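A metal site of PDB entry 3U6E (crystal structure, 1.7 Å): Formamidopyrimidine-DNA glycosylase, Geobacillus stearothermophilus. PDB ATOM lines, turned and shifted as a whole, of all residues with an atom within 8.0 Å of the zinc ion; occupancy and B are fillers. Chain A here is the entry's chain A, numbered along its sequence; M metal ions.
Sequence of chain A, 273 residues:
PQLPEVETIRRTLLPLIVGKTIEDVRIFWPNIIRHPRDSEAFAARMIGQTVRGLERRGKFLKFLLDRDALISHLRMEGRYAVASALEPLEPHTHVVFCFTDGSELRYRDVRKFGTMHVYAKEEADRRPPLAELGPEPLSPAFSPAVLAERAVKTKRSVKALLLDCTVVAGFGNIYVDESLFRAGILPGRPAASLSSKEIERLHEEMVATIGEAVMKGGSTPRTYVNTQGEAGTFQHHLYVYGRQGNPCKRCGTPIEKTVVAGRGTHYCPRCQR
The side-chain sulfur (SG) of Cys 268 lies close to the backbone NH (N) of Arg 270, at 3.4 Å.
The backbone NH (N) of Cys 268 lies within hydrogen-bond range of the side-chain amide oxygen (OE1) of Gln 272 (2.9 Å).
The backbone NH (N) of Arg 250 sits close to the side-chain sulfur (SG) of Cys 248, 3.3 Å away.
N of Cys 248 lies within hydrogen-bond range of O of Thr 253.
The side-chain sulfur of Cys 251 sits close to the side-chain hydroxyl of Thr 253, at 3.2 Å.
Four residues have an atom within 4 Å of the zinc ion: Cys 248, Cys 251, Cys 268 and Cys 271.
Along chain A the residues within 4 Å of the zinc ion span positions 248 to 271.
The zinc ion is bound by the side-chain sulfur of Cys 271 (2.3 Å), the side-chain sulfur of Cys 268 (2.3 Å), the side-chain sulfur of Cys 248 (2.4 Å) and the side-chain sulfur of Cys 251 (2.4 Å).
The zinc ion has four donor atoms within binding distance.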
ATOM      1  N   PHE A 181      29.254 -34.812 -18.036  1.00  0.00           N
ATOM      2  CA  PHE A 181      28.740 -34.076 -19.185  1.00  0.00           C
ATOM      3  C   PHE A 181      27.512 -34.779 -19.759  1.00  0.00           C
ATOM      4  O   PHE A 181      26.485 -34.162 -20.010  1.00  0.00           O
ATOM      5  CB  PHE A 181      29.794 -33.920 -20.277  1.00  0.00           C
ATOM      6  CG  PHE A 181      29.218 -33.420 -21.573  1.00  0.00           C
ATOM      7  CD1 PHE A 181      29.036 -32.060 -21.777  1.00  0.00           C
ATOM      8  CD2 PHE A 181      28.830 -34.311 -22.559  1.00  0.00           C
ATOM      9  CE1 PHE A 181      28.487 -31.595 -22.970  1.00  0.00           C
ATOM     10  CE2 PHE A 181      28.280 -33.856 -23.751  1.00  0.00           C
ATOM     11  CZ  PHE A 181      28.108 -32.487 -23.953  1.00  0.00           C
ATOM     12  N   TYR A 239      33.622 -35.664 -25.350  1.00  0.00           N
ATOM     13  CA  TYR A 239      32.780 -34.472 -25.377  1.00  0.00           C
ATOM     14  C   TYR A 239      33.450 -33.278 -24.706  1.00  0.00           C
ATOM     15  O   TYR A 239      33.303 -32.136 -25.159  1.00  0.00           O
ATOM     16  CB  TYR A 239      31.433 -34.732 -24.696  1.00  0.00           C
ATOM     17  CG  TYR A 239      30.527 -35.682 -25.433  1.00  0.00           C
ATOM     18  CD1 TYR A 239      30.364 -36.995 -25.004  1.00  0.00           C
ATOM     19  CD2 TYR A 239      29.841 -35.271 -26.571  1.00  0.00           C
ATOM     20  CE1 TYR A 239      29.538 -37.872 -25.680  1.00  0.00           C
ATOM     21  CE2 TYR A 239      29.008 -36.150 -27.259  1.00  0.00           C
ATOM     22  CZ  TYR A 239      28.857 -37.447 -26.798  1.00  0.00           C
ATOM     23  OH  TYR A 239      28.041 -38.315 -27.472  1.00  0.00           O
ATOM     24  N   VAL A 240      34.175 -33.531 -23.625  1.00  0.00           N
ATOM     25  CA  VAL A 240      34.727 -32.434 -22.840  1.00  0.00           C
ATOM     26  C   VAL A 240      36.192 -32.598 -22.451  1.00  0.00           C
ATOM     27  O   VAL A 240      36.957 -31.626 -22.439  1.00  0.00           O
ATOM     28  CB  VAL A 240      33.890 -32.169 -21.554  1.00  0.00           C
ATOM     29  CG1 VAL A 240      32.467 -31.781 -21.929  1.00  0.00           C
ATOM     30  CG2 VAL A 240      33.896 -33.385 -20.623  1.00  0.00           C
ATOM     31  N   PRO A 247      34.537 -25.827 -29.183  1.00  0.00           N
ATOM     32  CA  PRO A 247      33.073 -25.830 -29.060  1.00  0.00           C
ATOM     33  C   PRO A 247      32.519 -27.162 -28.567  1.00  0.00           C
ATOM     34  O   PRO A 247      32.971 -28.233 -28.969  1.00  0.00           O
ATOM     35  CB  PRO A 247      32.601 -25.565 -30.494  1.00  0.00           C
ATOM     36  CG  PRO A 247      33.758 -25.944 -31.364  1.00  0.00           C
ATOM     37  CD  PRO A 247      34.992 -25.662 -30.571  1.00  0.00           C
ATOM     38  N   CYS A 248      31.536 -27.068 -27.673  1.00  0.00           N
ATOM     39  CA  CYS A 248      30.810 -28.245 -27.237  1.00  0.00           C
ATOM     40  C   CYS A 248      30.206 -28.938 -28.456  1.00  0.00           C
ATOM     41  O   CYS A 248      29.681 -28.287 -29.363  1.00  0.00           O
ATOM     42  CB  CYS A 248      29.712 -27.852 -26.255  1.00  0.00           C
ATOM     43  SG  CYS A 248      28.623 -29.210 -25.773  1.00  0.00           S
ATOM     44  N   LYS A 249      30.290 -30.270 -28.493  1.00  0.00           N
ATOM     45  CA  LYS A 249      29.778 -31.030 -29.624  1.00  0.00           C
ATOM     46  C   LYS A 249      28.255 -31.097 -29.655  1.00  0.00           C
ATOM     47  O   LYS A 249      27.662 -31.503 -30.658  1.00  0.00           O
ATOM     48  CB  LYS A 249      30.361 -32.450 -29.624  1.00  0.00           C
ATOM     49  CG  LYS A 249      31.865 -32.478 -29.780  1.00  0.00           C
ATOM     50  CD  LYS A 249      32.402 -33.890 -29.926  1.00  0.00           C
ATOM     51  CE  LYS A 249      33.912 -33.870 -30.092  1.00  0.00           C
ATOM     52  NZ  LYS A 249      34.483 -35.240 -30.269  1.00  0.00           N
ATOM     53  N   ARG A 250      27.614 -30.698 -28.553  1.00  0.00           N
ATOM     54  CA  ARG A 250      26.156 -30.702 -28.482  1.00  0.00           C
ATOM     55  C   ARG A 250      25.545 -29.306 -28.625  1.00  0.00           C
ATOM     56  O   ARG A 250      24.449 -29.175 -29.149  1.00  0.00           O
ATOM     57  CB  ARG A 250      25.666 -31.362 -27.182  1.00  0.00           C
ATOM     58  CG  ARG A 250      26.002 -32.844 -27.084  1.00  0.00           C
ATOM     59  CD  ARG A 250      24.788 -33.654 -26.662  1.00  0.00           C
ATOM     60  NE  ARG A 250      25.060 -35.083 -26.650  1.00  0.00           N
ATOM     61  CZ  ARG A 250      25.112 -35.818 -25.538  1.00  0.00           C
ATOM     62  NH1 ARG A 250      24.899 -35.264 -24.360  1.00  0.00           N
ATOM     63  NH2 ARG A 250      25.372 -37.121 -25.624  1.00  0.00           N
ATOM     64  N   CYS A 251      26.245 -28.276 -28.143  1.00  0.00           N
ATOM     65  CA  CYS A 251      25.640 -26.949 -28.159  1.00  0.00           C
ATOM     66  C   CYS A 251      26.526 -25.835 -28.712  1.00  0.00           C
ATOM     67  O   CYS A 251      26.052 -24.714 -28.909  1.00  0.00           O
ATOM     68  CB  CYS A 251      25.144 -26.562 -26.763  1.00  0.00           C
ATOM     69  SG  CYS A 251      26.459 -26.070 -25.629  1.00  0.00           S
ATOM     70  N   GLY A 252      27.793 -26.123 -28.935  1.00  0.00           N
ATOM     71  CA  GLY A 252      28.700 -25.151 -29.513  1.00  0.00           C
ATOM     72  C   GLY A 252      29.339 -24.170 -28.534  1.00  0.00           C
ATOM     73  O   GLY A 252      30.202 -23.381 -28.921  1.00  0.00           O
ATOM     74  N   THR A 253      28.902 -24.209 -27.276  1.00  0.00           N
ATOM     75  CA  THR A 253      29.474 -23.353 -26.246  1.00  0.00           C
ATOM     76  C   THR A 253      30.917 -23.805 -25.978  1.00  0.00           C
ATOM     77  O   THR A 253      31.188 -25.004 -25.946  1.00  0.00           O
ATOM     78  CB  THR A 253      28.668 -23.468 -24.936  1.00  0.00           C
ATOM     79  OG1 THR A 253      27.318 -23.053 -25.176  1.00  0.00           O
ATOM     80  CG2 THR A 253      29.292 -22.596 -23.839  1.00  0.00           C
ATOM     81  N   PRO A 254      31.846 -22.852 -25.793  1.00  0.00           N
ATOM     82  CA  PRO A 254      33.213 -23.281 -25.512  1.00  0.00           C
ATOM     83  C   PRO A 254      33.323 -24.106 -24.243  1.00  0.00           C
ATOM     84  O   PRO A 254      32.826 -23.705 -23.193  1.00  0.00           O
ATOM     85  CB  PRO A 254      33.969 -21.958 -25.338  1.00  0.00           C
ATOM     86  CG  PRO A 254      33.190 -20.977 -26.145  1.00  0.00           C
ATOM     87  CD  PRO A 254      31.749 -21.403 -26.013  1.00  0.00           C
ATOM     88  N   ILE A 255      33.966 -25.255 -24.341  1.00  0.00           N
ATOM     89  CA  ILE A 255      34.233 -26.077 -23.163  1.00  0.00           C
ATOM     90  C   ILE A 255      35.195 -25.336 -22.252  1.00  0.00           C
ATOM     91  O   ILE A 255      36.119 -24.651 -22.715  1.00  0.00           O
ATOM     92  CB  ILE A 255      34.837 -27.435 -23.569  1.00  0.00           C
ATOM     93  CG1 ILE A 255      33.855 -28.184 -24.484  1.00  0.00           C
ATOM     94  CG2 ILE A 255      35.176 -28.264 -22.324  1.00  0.00           C
ATOM     95  CD1 ILE A 255      32.440 -28.273 -23.918  1.00  0.00           C
ATOM     96  N   TYR A 267      34.189 -29.154 -18.623  1.00  0.00           N
ATOM     97  CA  TYR A 267      32.735 -29.184 -18.631  1.00  0.00           C
ATOM     98  C   TYR A 267      32.184 -28.164 -19.611  1.00  0.00           C
ATOM     99  O   TYR A 267      32.870 -27.219 -20.005  1.00  0.00           O
ATOM    100  CB  TYR A 267      32.210 -28.896 -17.231  1.00  0.00           C
ATOM    101  CG  TYR A 267      32.569 -27.511 -16.734  1.00  0.00           C
ATOM    102  CD1 TYR A 267      31.722 -26.434 -16.929  1.00  0.00           C
ATOM    103  CD2 TYR A 267      33.788 -27.277 -16.097  1.00  0.00           C
ATOM    104  CE1 TYR A 267      32.050 -25.169 -16.490  1.00  0.00           C
ATOM    105  CE2 TYR A 267      34.135 -26.013 -15.651  1.00  0.00           C
ATOM    106  CZ  TYR A 267      33.260 -24.956 -15.861  1.00  0.00           C
ATOM    107  OH  TYR A 267      33.588 -23.691 -15.421  1.00  0.00           O
ATOM    108  N   CYS A 268      30.932 -28.358 -20.011  1.00  0.00           N
ATOM    109  CA  CYS A 268      30.228 -27.360 -20.787  1.00  0.00           C
ATOM    110  C   CYS A 268      29.284 -26.616 -19.851  1.00  0.00           C
ATOM    111  O   CYS A 268      28.417 -27.235 -19.225  1.00  0.00           O
ATOM    112  CB  CYS A 268      29.439 -28.001 -21.915  1.00  0.00           C
ATOM    113  SG  CYS A 268      28.374 -26.813 -22.741  1.00  0.00           S
ATOM    114  N   PRO A 269      29.454 -25.294 -19.753  1.00  0.00           N
ATOM    115  CA  PRO A 269      28.666 -24.469 -18.829  1.00  0.00           C
ATOM    116  C   PRO A 269      27.214 -24.336 -19.261  1.00  0.00           C
ATOM    117  O   PRO A 269      26.412 -23.825 -18.482  1.00  0.00           O
ATOM    118  CB  PRO A 269      29.378 -23.121 -18.868  1.00  0.00           C
ATOM    119  CG  PRO A 269      30.039 -23.073 -20.197  1.00  0.00           C
ATOM    120  CD  PRO A 269      30.402 -24.494 -20.556  1.00  0.00           C
ATOM    121  N   ARG A 270      26.872 -24.792 -20.463  1.00  0.00           N
ATOM    122  CA  ARG A 270      25.487 -24.755 -20.926  1.00  0.00           C
ATOM    123  C   ARG A 270      24.762 -26.085 -20.745  1.00  0.00           C
ATOM    124  O   ARG A 270      23.647 -26.126 -20.215  1.00  0.00           O
ATOM    125  CB  ARG A 270      25.394 -24.297 -22.384  1.00  0.00           C
ATOM    126  CG  ARG A 270      23.957 -24.165 -22.864  1.00  0.00           C
ATOM    127  CD  ARG A 270      23.861 -23.683 -24.306  1.00  0.00           C
ATOM    128  NE  ARG A 270      22.460 -23.592 -24.712  1.00  0.00           N
ATOM    129  CZ  ARG A 270      22.026 -23.059 -25.853  1.00  0.00           C
ATOM    130  NH1 ARG A 270      20.732 -23.026 -26.115  1.00  0.00           N
ATOM    131  NH2 ARG A 270      22.884 -22.560 -26.732  1.00  0.00           N
ATOM    132  N   CYS A 271      25.384 -27.174 -21.187  1.00  0.00           N
ATOM    133  CA  CYS A 271      24.783 -28.506 -21.095  1.00  0.00           C
ATOM    134  C   CYS A 271      24.730 -29.032 -19.657  1.00  0.00           C
ATOM    135  O   CYS A 271      23.859 -29.828 -19.313  1.00  0.00           O
ATOM    136  CB  CYS A 271      25.556 -29.511 -21.949  1.00  0.00           C
ATOM    137  SG  CYS A 271      25.431 -29.256 -23.733  1.00  0.00           S
ATOM    138  N   GLN A 272      25.669 -28.592 -18.833  1.00  0.00           N
ATOM    139  CA  GLN A 272      25.767 -29.088 -17.462  1.00  0.00           C
ATOM    140  C   GLN A 272      25.256 -28.049 -16.469  1.00  0.00           C
ATOM    141  O   GLN A 272      25.527 -26.859 -16.610  1.00  0.00           O
ATOM    142  CB  GLN A 272      27.200 -29.500 -17.153  1.00  0.00           C
ATOM    143  CG  GLN A 272      27.629 -30.733 -17.933  1.00  0.00           C
ATOM    144  CD  GLN A 272      29.114 -31.011 -17.854  1.00  0.00           C
ATOM    145  OE1 GLN A 272      29.859 -30.701 -18.778  1.00  0.00           O
ATOM    146  NE2 GLN A 272      29.546 -31.613 -16.751  1.00  0.00           N
HETATM  147 ZN    ZN M   1      27.176 -27.955 -24.394  1.00  0.00          ZN
